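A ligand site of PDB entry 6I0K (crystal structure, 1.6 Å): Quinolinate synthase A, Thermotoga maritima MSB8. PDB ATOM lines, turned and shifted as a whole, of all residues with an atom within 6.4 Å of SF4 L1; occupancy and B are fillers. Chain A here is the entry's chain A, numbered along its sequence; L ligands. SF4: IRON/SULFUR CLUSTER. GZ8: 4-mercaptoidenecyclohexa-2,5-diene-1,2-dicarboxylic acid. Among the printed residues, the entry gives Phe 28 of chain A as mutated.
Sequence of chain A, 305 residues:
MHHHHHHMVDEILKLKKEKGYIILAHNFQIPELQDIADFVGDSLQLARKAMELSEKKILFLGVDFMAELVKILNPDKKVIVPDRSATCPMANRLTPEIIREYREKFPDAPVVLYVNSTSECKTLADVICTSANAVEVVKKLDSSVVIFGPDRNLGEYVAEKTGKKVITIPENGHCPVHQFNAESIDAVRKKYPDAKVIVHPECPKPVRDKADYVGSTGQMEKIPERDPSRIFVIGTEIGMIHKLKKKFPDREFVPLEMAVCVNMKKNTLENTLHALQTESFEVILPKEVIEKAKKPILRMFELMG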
ATOM      1  N   HIS A  26       9.120   7.523 -26.041  1.00  0.00           N
ATOM      2  CA  HIS A  26       8.772   7.948 -24.667  1.00  0.00           C
ATOM      3  C   HIS A  26       7.254   8.085 -24.515  1.00  0.00           C
ATOM      4  O   HIS A  26       6.539   8.391 -25.498  1.00  0.00           O
ATOM      5  CB  HIS A  26       9.489   9.250 -24.302  1.00  0.00           C
ATOM      6  CG  HIS A  26       9.343   9.571 -22.855  1.00  0.00           C
ATOM      7  ND1 HIS A  26       8.385  10.459 -22.392  1.00  0.00           N
ATOM      8  CD2 HIS A  26      10.010   9.128 -21.767  1.00  0.00           C
ATOM      9  CE1 HIS A  26       8.461  10.535 -21.088  1.00  0.00           C
ATOM     10  NE2 HIS A  26       9.458   9.735 -20.672  1.00  0.00           N
ATOM     11  N   PHE A  28       5.623  10.480 -23.506  1.00  0.00           N
ATOM     12  CA  PHE A  28       5.120  11.854 -23.796  1.00  0.00           C
ATOM     13  C   PHE A  28       5.083  12.151 -25.302  1.00  0.00           C
ATOM     14  O   PHE A  28       4.811  13.308 -25.681  1.00  0.00           O
ATOM     15  CB  PHE A  28       5.953  12.901 -23.054  1.00  0.00           C
ATOM     16  CG  PHE A  28       5.879  12.848 -21.545  1.00  0.00           C
ATOM     17  CD1 PHE A  28       4.928  12.074 -20.887  1.00  0.00           C
ATOM     18  CD2 PHE A  28       6.772  13.569 -20.777  1.00  0.00           C
ATOM     19  CE1 PHE A  28       4.869  12.039 -19.503  1.00  0.00           C
ATOM     20  CE2 PHE A  28       6.714  13.534 -19.393  1.00  0.00           C
ATOM     21  CZ  PHE A  28       5.770  12.757 -18.758  1.00  0.00           C
ATOM     22  N   VAL A  63      13.438  13.168 -26.088  1.00  0.00           N
ATOM     23  CA  VAL A  63      14.332  14.365 -26.034  1.00  0.00           C
ATOM     24  C   VAL A  63      15.778  13.910 -25.820  1.00  0.00           C
ATOM     25  O   VAL A  63      16.035  12.715 -25.535  1.00  0.00           O
ATOM     26  CB  VAL A  63      13.884  15.404 -24.988  1.00  0.00           C
ATOM     27  CG1 VAL A  63      12.509  15.955 -25.313  1.00  0.00           C
ATOM     28  CG2 VAL A  63      13.942  14.870 -23.557  1.00  0.00           C
ATOM     29  N   PHE A  65      18.380  14.032 -23.772  1.00  0.00           N
ATOM     30  CA  PHE A  65      19.049  13.388 -22.608  1.00  0.00           C
ATOM     31  C   PHE A  65      18.670  11.910 -22.579  1.00  0.00           C
ATOM     32  O   PHE A  65      19.493  11.091 -22.153  1.00  0.00           O
ATOM     33  CB  PHE A  65      18.728  14.065 -21.270  1.00  0.00           C
ATOM     34  CG  PHE A  65      17.352  13.802 -20.707  1.00  0.00           C
ATOM     35  CD1 PHE A  65      17.025  12.586 -20.123  1.00  0.00           C
ATOM     36  CD2 PHE A  65      16.379  14.788 -20.755  1.00  0.00           C
ATOM     37  CE1 PHE A  65      15.770  12.353 -19.612  1.00  0.00           C
ATOM     38  CE2 PHE A  65      15.116  14.557 -20.238  1.00  0.00           C
ATOM     39  CZ  PHE A  65      14.805  13.337 -19.666  1.00  0.00           C
ATOM     40  N   MET A  66      17.465  11.574 -23.063  1.00  0.00           N
ATOM     41  CA  MET A  66      16.968  10.180 -23.107  1.00  0.00           C
ATOM     42  C   MET A  66      17.658   9.415 -24.231  1.00  0.00           C
ATOM     43  O   MET A  66      18.058   8.227 -24.049  1.00  0.00           O
ATOM     44  CB  MET A  66      15.479  10.119 -23.403  1.00  0.00           C
ATOM     45  CG  MET A  66      14.636  10.984 -22.561  1.00  0.00           C
ATOM     46  SD  MET A  66      12.909  10.743 -22.999  1.00  0.00           S
ATOM     47  CE  MET A  66      12.279  11.622 -21.570  1.00  0.00           C
ATOM     48  N   THR A  87      14.928  18.767 -26.547  1.00  0.00           N
ATOM     49  CA  THR A  87      15.780  18.870 -25.349  1.00  0.00           C
ATOM     50  C   THR A  87      14.878  19.111 -24.133  1.00  0.00           C
ATOM     51  O   THR A  87      13.677  19.299 -24.296  1.00  0.00           O
ATOM     52  CB  THR A  87      16.806  19.990 -25.555  1.00  0.00           C
ATOM     53  OG1 THR A  87      17.880  19.810 -24.629  1.00  0.00           O
ATOM     54  CG2 THR A  87      16.196  21.379 -25.403  1.00  0.00           C
ATOM     55  N   CYS A  88      15.465  19.092 -22.944  1.00  0.00           N
ATOM     56  CA  CYS A  88      14.743  19.387 -21.692  1.00  0.00           C
ATOM     57  C   CYS A  88      15.219  20.735 -21.172  1.00  0.00           C
ATOM     58  O   CYS A  88      16.339  20.847 -20.689  1.00  0.00           O
ATOM     59  CB  CYS A  88      14.969  18.282 -20.662  1.00  0.00           C
ATOM     60  SG  CYS A  88      14.244  18.687 -19.051  1.00  0.00           S
ATOM     61  N   PRO A  89      14.406  21.808 -21.292  1.00  0.00           N
ATOM     62  CA  PRO A  89      14.830  23.095 -20.751  1.00  0.00           C
ATOM     63  C   PRO A  89      15.181  23.011 -19.253  1.00  0.00           C
ATOM     64  O   PRO A  89      16.062  23.725 -18.850  1.00  0.00           O
ATOM     65  CB  PRO A  89      13.632  24.000 -21.013  1.00  0.00           C
ATOM     66  CG  PRO A  89      13.000  23.395 -22.230  1.00  0.00           C
ATOM     67  CD  PRO A  89      13.120  21.907 -21.995  1.00  0.00           C
ATOM     68  N   MET A  90      14.550  22.124 -18.477  1.00  0.00           N
ATOM     69  CA  MET A  90      14.869  21.973 -17.034  1.00  0.00           C
ATOM     70  C   MET A  90      16.289  21.416 -16.871  1.00  0.00           C
ATOM     71  O   MET A  90      17.088  22.000 -16.113  1.00  0.00           O
ATOM     72  CB  MET A  90      13.869  21.058 -16.305  1.00  0.00           C
ATOM     73  CG  MET A  90      14.197  20.845 -14.826  1.00  0.00           C
ATOM     74  SD  MET A  90      13.216  19.510 -14.076  1.00  0.00           S
ATOM     75  CE  MET A  90      13.973  18.083 -14.849  1.00  0.00           C
ATOM     76  N   ALA A  91      16.601  20.315 -17.558  1.00  0.00           N
ATOM     77  CA  ALA A  91      17.950  19.725 -17.518  1.00  0.00           C
ATOM     78  C   ALA A  91      18.977  20.824 -17.839  1.00  0.00           C
ATOM     79  O   ALA A  91      20.011  20.918 -17.154  1.00  0.00           O
ATOM     80  CB  ALA A  91      18.044  18.558 -18.467  1.00  0.00           C
ATOM     81  N   TYR A 114      19.111  13.716 -11.074  1.00  0.00           N
ATOM     82  CA  TYR A 114      17.890  13.209 -11.729  1.00  0.00           C
ATOM     83  C   TYR A 114      18.290  12.896 -13.176  1.00  0.00           C
ATOM     84  O   TYR A 114      19.088  13.647 -13.758  1.00  0.00           O
ATOM     85  CB  TYR A 114      16.805  14.269 -11.574  1.00  0.00           C
ATOM     86  CG  TYR A 114      15.441  13.924 -12.118  1.00  0.00           C
ATOM     87  CD1 TYR A 114      14.979  12.616 -12.178  1.00  0.00           C
ATOM     88  CD2 TYR A 114      14.589  14.931 -12.532  1.00  0.00           C
ATOM     89  CE1 TYR A 114      13.708  12.322 -12.648  1.00  0.00           C
ATOM     90  CE2 TYR A 114      13.311  14.651 -13.015  1.00  0.00           C
ATOM     91  CZ  TYR A 114      12.876  13.330 -13.086  1.00  0.00           C
ATOM     92  OH  TYR A 114      11.630  13.044 -13.574  1.00  0.00           O
ATOM     93  N   ASN A 116      16.786  13.268 -15.769  1.00  0.00           N
ATOM     94  CA  ASN A 116      16.440  14.473 -16.565  1.00  0.00           C
ATOM     95  C   ASN A 116      17.540  15.496 -16.285  1.00  0.00           C
ATOM     96  O   ASN A 116      17.291  16.438 -15.504  1.00  0.00           O
ATOM     97  CB  ASN A 116      15.034  14.993 -16.258  1.00  0.00           C
ATOM     98  CG  ASN A 116      13.928  13.961 -16.439  1.00  0.00           C
ATOM     99  OD1 ASN A 116      14.147  12.738 -16.319  1.00  0.00           O
ATOM    100  ND2 ASN A 116      12.701  14.434 -16.671  1.00  0.00           N
ATOM    101  N   ASP A 151      15.737  19.186 -10.490  1.00  0.00           N
ATOM    102  CA  ASP A 151      14.331  19.489 -10.122  1.00  0.00           C
ATOM    103  C   ASP A 151      14.222  19.695  -8.615  1.00  0.00           C
ATOM    104  O   ASP A 151      14.429  18.718  -7.867  1.00  0.00           O
ATOM    105  CB  ASP A 151      13.397  18.371 -10.592  1.00  0.00           C
ATOM    106  CG  ASP A 151      11.929  18.771 -10.520  1.00  0.00           C
ATOM    107  OD1 ASP A 151      11.436  18.975  -9.389  1.00  0.00           O
ATOM    108  OD2 ASP A 151      11.300  18.884 -11.592  1.00  0.00           O
ATOM    109  N   HIS A 174      13.011  23.460 -11.949  1.00  0.00           N
ATOM    110  CA  HIS A 174      11.636  22.910 -12.066  1.00  0.00           C
ATOM    111  C   HIS A 174      11.252  22.637 -13.515  1.00  0.00           C
ATOM    112  O   HIS A 174      11.810  23.265 -14.439  1.00  0.00           O
ATOM    113  CB  HIS A 174      10.609  23.882 -11.484  1.00  0.00           C
ATOM    114  CG  HIS A 174      10.377  25.049 -12.371  1.00  0.00           C
ATOM    115  ND1 HIS A 174      11.213  26.146 -12.379  1.00  0.00           N
ATOM    116  CD2 HIS A 174       9.444  25.272 -13.328  1.00  0.00           C
ATOM    117  CE1 HIS A 174      10.797  27.011 -13.273  1.00  0.00           C
ATOM    118  NE2 HIS A 174       9.719  26.493 -13.882  1.00  0.00           N
ATOM    119  N   CYS A 175      10.248  21.789 -13.656  1.00  0.00           N
ATOM    120  CA  CYS A 175       9.632  21.418 -14.937  1.00  0.00           C
ATOM    121  C   CYS A 175       8.386  22.264 -15.103  1.00  0.00           C
ATOM    122  O   CYS A 175       7.461  22.147 -14.298  1.00  0.00           O
ATOM    123  CB  CYS A 175       9.268  19.934 -14.938  1.00  0.00           C
ATOM    124  SG  CYS A 175       8.320  19.489 -16.407  1.00  0.00           S
ATOM    125  N   PRO A 176       8.314  23.130 -16.149  1.00  0.00           N
ATOM    126  CA  PRO A 176       7.131  23.957 -16.377  1.00  0.00           C
ATOM    127  C   PRO A 176       5.868  23.116 -16.636  1.00  0.00           C
ATOM    128  O   PRO A 176       4.774  23.527 -16.310  1.00  0.00           O
ATOM    129  CB  PRO A 176       7.460  24.761 -17.650  1.00  0.00           C
ATOM    130  CG  PRO A 176       8.945  24.604 -17.839  1.00  0.00           C
ATOM    131  CD  PRO A 176       9.321  23.287 -17.205  1.00  0.00           C
ATOM    132  N   VAL A 177       6.044  21.917 -17.199  1.00  0.00           N
ATOM    133  CA  VAL A 177       4.909  21.049 -17.619  1.00  0.00           C
ATOM    134  C   VAL A 177       4.116  20.625 -16.378  1.00  0.00           C
ATOM    135  O   VAL A 177       2.873  20.526 -16.459  1.00  0.00           O
ATOM    136  CB  VAL A 177       5.410  19.862 -18.451  1.00  0.00           C
ATOM    137  CG1 VAL A 177       4.302  18.890 -18.796  1.00  0.00           C
ATOM    138  CG2 VAL A 177       6.115  20.334 -19.725  1.00  0.00           C
ATOM    139  N   HIS A 178       4.780  20.426 -15.244  1.00  0.00           N
ATOM    140  CA  HIS A 178       4.166  19.815 -14.036  1.00  0.00           C
ATOM    141  C   HIS A 178       3.703  20.886 -13.040  1.00  0.00           C
ATOM    142  O   HIS A 178       3.302  20.499 -11.933  1.00  0.00           O
ATOM    143  CB  HIS A 178       5.144  18.814 -13.399  1.00  0.00           C
ATOM    144  CG  HIS A 178       5.228  17.540 -14.166  1.00  0.00           C
ATOM    145  ND1 HIS A 178       6.209  17.310 -15.116  1.00  0.00           N
ATOM    146  CD2 HIS A 178       4.421  16.464 -14.178  1.00  0.00           C
ATOM    147  CE1 HIS A 178       6.010  16.128 -15.662  1.00  0.00           C
ATOM    148  NE2 HIS A 178       4.922  15.590 -15.105  1.00  0.00           N
ATOM    149  N   GLU A 202       7.295  15.724  -9.547  1.00  0.00           N
ATOM    150  CA  GLU A 202       7.796  17.008 -10.090  1.00  0.00           C
ATOM    151  C   GLU A 202       6.746  18.105  -9.883  1.00  0.00           C
ATOM    152  O   GLU A 202       7.063  19.292 -10.067  1.00  0.00           O
ATOM    153  CB  GLU A 202       8.187  16.881 -11.565  1.00  0.00           C
ATOM    154  CG  GLU A 202       9.498  16.147 -11.751  1.00  0.00           C
ATOM    155  CD  GLU A 202      10.073  16.148 -13.158  1.00  0.00           C
ATOM    156  OE1 GLU A 202      10.580  17.182 -13.618  1.00  0.00           O
ATOM    157  OE2 GLU A 202      10.039  15.102 -13.770  1.00  0.00           O
ATOM    158  N   GLU A 237       2.287  14.998 -18.131  1.00  0.00           N
ATOM    159  CA  GLU A 237       2.212  15.435 -19.549  1.00  0.00           C
ATOM    160  C   GLU A 237       1.117  14.632 -20.269  1.00  0.00           C
ATOM    161  O   GLU A 237       0.965  13.418 -20.004  1.00  0.00           O
ATOM    162  CB  GLU A 237       3.597  15.266 -20.206  1.00  0.00           C
ATOM    163  CG  GLU A 237       3.885  16.250 -21.319  1.00  0.00           C
ATOM    164  CD  GLU A 237       3.444  15.794 -22.693  1.00  0.00           C
ATOM    165  OE1 GLU A 237       3.051  14.616 -22.828  1.00  0.00           O
ATOM    166  OE2 GLU A 237       3.520  16.604 -23.635  1.00  0.00           O
ATOM    167  N   CYS A 261       4.571  19.196 -23.188  1.00  0.00           N
ATOM    168  CA  CYS A 261       6.027  19.445 -23.286  1.00  0.00           C
ATOM    169  C   CYS A 261       6.316  19.807 -24.749  1.00  0.00           C
ATOM    170  O   CYS A 261       6.247  18.917 -25.606  1.00  0.00           O
ATOM    171  CB  CYS A 261       6.833  18.213 -22.891  1.00  0.00           C
ATOM    172  SG  CYS A 261       8.616  18.535 -22.998  1.00  0.00           S
ATOM    173  N   VAL A 262       6.598  21.075 -25.029  1.00  0.00           N
ATOM    174  CA  VAL A 262       6.766  21.530 -26.431  1.00  0.00           C
ATOM    175  C   VAL A 262       7.900  20.724 -27.099  1.00  0.00           C
ATOM    176  O   VAL A 262       7.801  20.398 -28.291  1.00  0.00           O
ATOM    177  CB  VAL A 262       7.017  23.052 -26.462  1.00  0.00           C
ATOM    178  CG1 VAL A 262       7.539  23.540 -27.805  1.00  0.00           C
ATOM    179  CG2 VAL A 262       5.744  23.796 -26.086  1.00  0.00           C
ATOM    180  N   ASN A 263       8.951  20.411 -26.349  1.00  0.00           N
ATOM    181  CA  ASN A 263      10.107  19.663 -26.920  1.00  0.00           C
ATOM    182  C   ASN A 263       9.694  18.249 -27.294  1.00  0.00           C
ATOM    183  O   ASN A 263      10.097  17.786 -28.368  1.00  0.00           O
ATOM    184  CB  ASN A 263      11.288  19.671 -25.966  1.00  0.00           C
ATOM    185  CG  ASN A 263      12.149  20.889 -26.193  1.00  0.00           C
ATOM    186  OD1 ASN A 263      13.016  20.884 -27.069  1.00  0.00           O
ATOM    187  ND2 ASN A 263      11.909  21.931 -25.418  1.00  0.00           N
ATOM    188  N   MET A 264       8.911  17.585 -26.460  1.00  0.00           N
ATOM    189  CA  MET A 264       8.418  16.217 -26.751  1.00  0.00           C
ATOM    190  C   MET A 264       7.576  16.217 -28.044  1.00  0.00           C
ATOM    191  O   MET A 264       7.631  15.232 -28.799  1.00  0.00           O
ATOM    192  CB  MET A 264       7.578  15.682 -25.589  1.00  0.00           C
ATOM    193  CG  MET A 264       8.405  15.208 -24.408  1.00  0.00           C
ATOM    194  SD  MET A 264       9.322  13.701 -24.790  1.00  0.00           S
ATOM    195  CE  MET A 264      10.140  13.511 -23.200  1.00  0.00           C
HETATM  196 FE1  SF4 L   1       9.499  18.593 -18.084  1.00  0.00          FE
HETATM  197 FE2  SF4 L   1       9.640  18.302 -20.878  1.00  0.00          FE
HETATM  198 FE3  SF4 L   1      10.301  16.224 -19.168  1.00  0.00          FE
HETATM  199 FE4  SF4 L   1      11.953  18.323 -19.354  1.00  0.00          FE
HETATM  200  S1  SF4 L   1      11.532  16.920 -21.107  1.00  0.00           S
HETATM  201  S2  SF4 L   1      11.268  17.211 -17.380  1.00  0.00           S
HETATM  202  S3  SF4 L   1      10.440  20.143 -19.667  1.00  0.00           S
HETATM  203  S4  SF4 L   1       8.184  17.228 -19.325  1.00  0.00           S
HETATM  204  O3  GZ8 L   2       8.757   8.782 -15.978  1.00  0.00           O
HETATM  205  C8  GZ8 L   2       8.749   9.939 -15.519  1.00  0.00           C
HETATM  206  O4  GZ8 L   2       8.045  10.097 -14.524  1.00  0.00           O
HETATM  207  C3  GZ8 L   2       9.340  11.025 -16.371  1.00  0.00           C
HETATM  208  C2  GZ8 L   2      10.339  10.750 -17.316  1.00  0.00           C
HETATM  209  C7  GZ8 L   2      11.057   9.440 -17.433  1.00  0.00           C
HETATM  210  O2  GZ8 L   2      11.170   8.903 -18.516  1.00  0.00           O
HETATM  211  O1  GZ8 L   2      11.588   8.925 -16.421  1.00  0.00           O
HETATM  212  C4  GZ8 L   2       8.799  12.305 -16.364  1.00  0.00           C
HETATM  213  C5  GZ8 L   2       9.234  13.279 -17.234  1.00  0.00           C
HETATM  214  C6  GZ8 L   2      10.215  12.973 -18.158  1.00  0.00           C
HETATM  215  C1  GZ8 L   2      10.769  11.719 -18.174  1.00  0.00           C
HETATM  216  S   GZ8 L   2      10.770  14.038 -19.349  1.00  0.00           S
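Merely in contact with SF4 L1: Val 177, Met 90, Glu 202, Pro 89 and Phe 28. Nine residues have an atom within 4 Å of SF4 L1: Phe 28, Cys 88, Pro 89, Met 90, Asn 116, Cys 175, Val 177, Glu 202 and Cys 261. Along chain A the residues within 4 Å of SF4 L1 span positions 28 to 261. The nearest printed residue that does not touch SF4 L1 is Val 63 (4.002 Å).
The side-chain sulfur of Cys 261 binds an iron atom (FE2) of SF4 L1 (2.4 Å). ND2 of Asn 116 lies close to S of GZ8 L2, at 3.3 Å. The side-chain amide nitrogen of Asn 116 lies close to a sulfur (S2) of SF4 L1 (3.2 Å). An iron atom (FE1) of SF4 L1 is bound by the side-chain sulfur (SG) of Cys 175, 2.2 Å away. A ring nitrogen (NE2) of His 26 lies within hydrogen-bond range of an oxygen (O2) of GZ8 L2. The side-chain sulfur of Cys 88 binds an iron atom (FE4) of SF4 L1 (2.3 Å).
A sulfur (S) of GZ8 L2 is bound to an iron atom (FE3) of SF4 L1.
The side-chain sulfur of Cys 175 sits close to a ring nitrogen (ND1) of His 178 (3.3 Å). The side-chain hydroxyl (OH) of Tyr 114 lies within hydrogen-bond range of the side-chain carboxylate (OE2) of Glu 202 (2.6 Å). The backbone NH (N) of Cys 261 sits at hydrogen-bond distance from the side-chain carboxylate (OE2) of Glu 237 (2.8 Å). N of Val 177 sits close to SG of Cys 175, at 3.4 Å. SG of Cys 88 lies close to N of Met 90 (3.5 Å). The side-chain carboxylate of Asp 151 lies close to the side-chain carboxylate of Glu 202 (2.7 Å). The backbone NH (N) of Ala 91 lies close to the side-chain sulfur (SG) of Cys 88 (3.2 Å). The side-chain sulfur (SD) of Met 90 sits at hydrogen-bond distance from the backbone NH (N) of Cys 175, 3.8 Å away.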
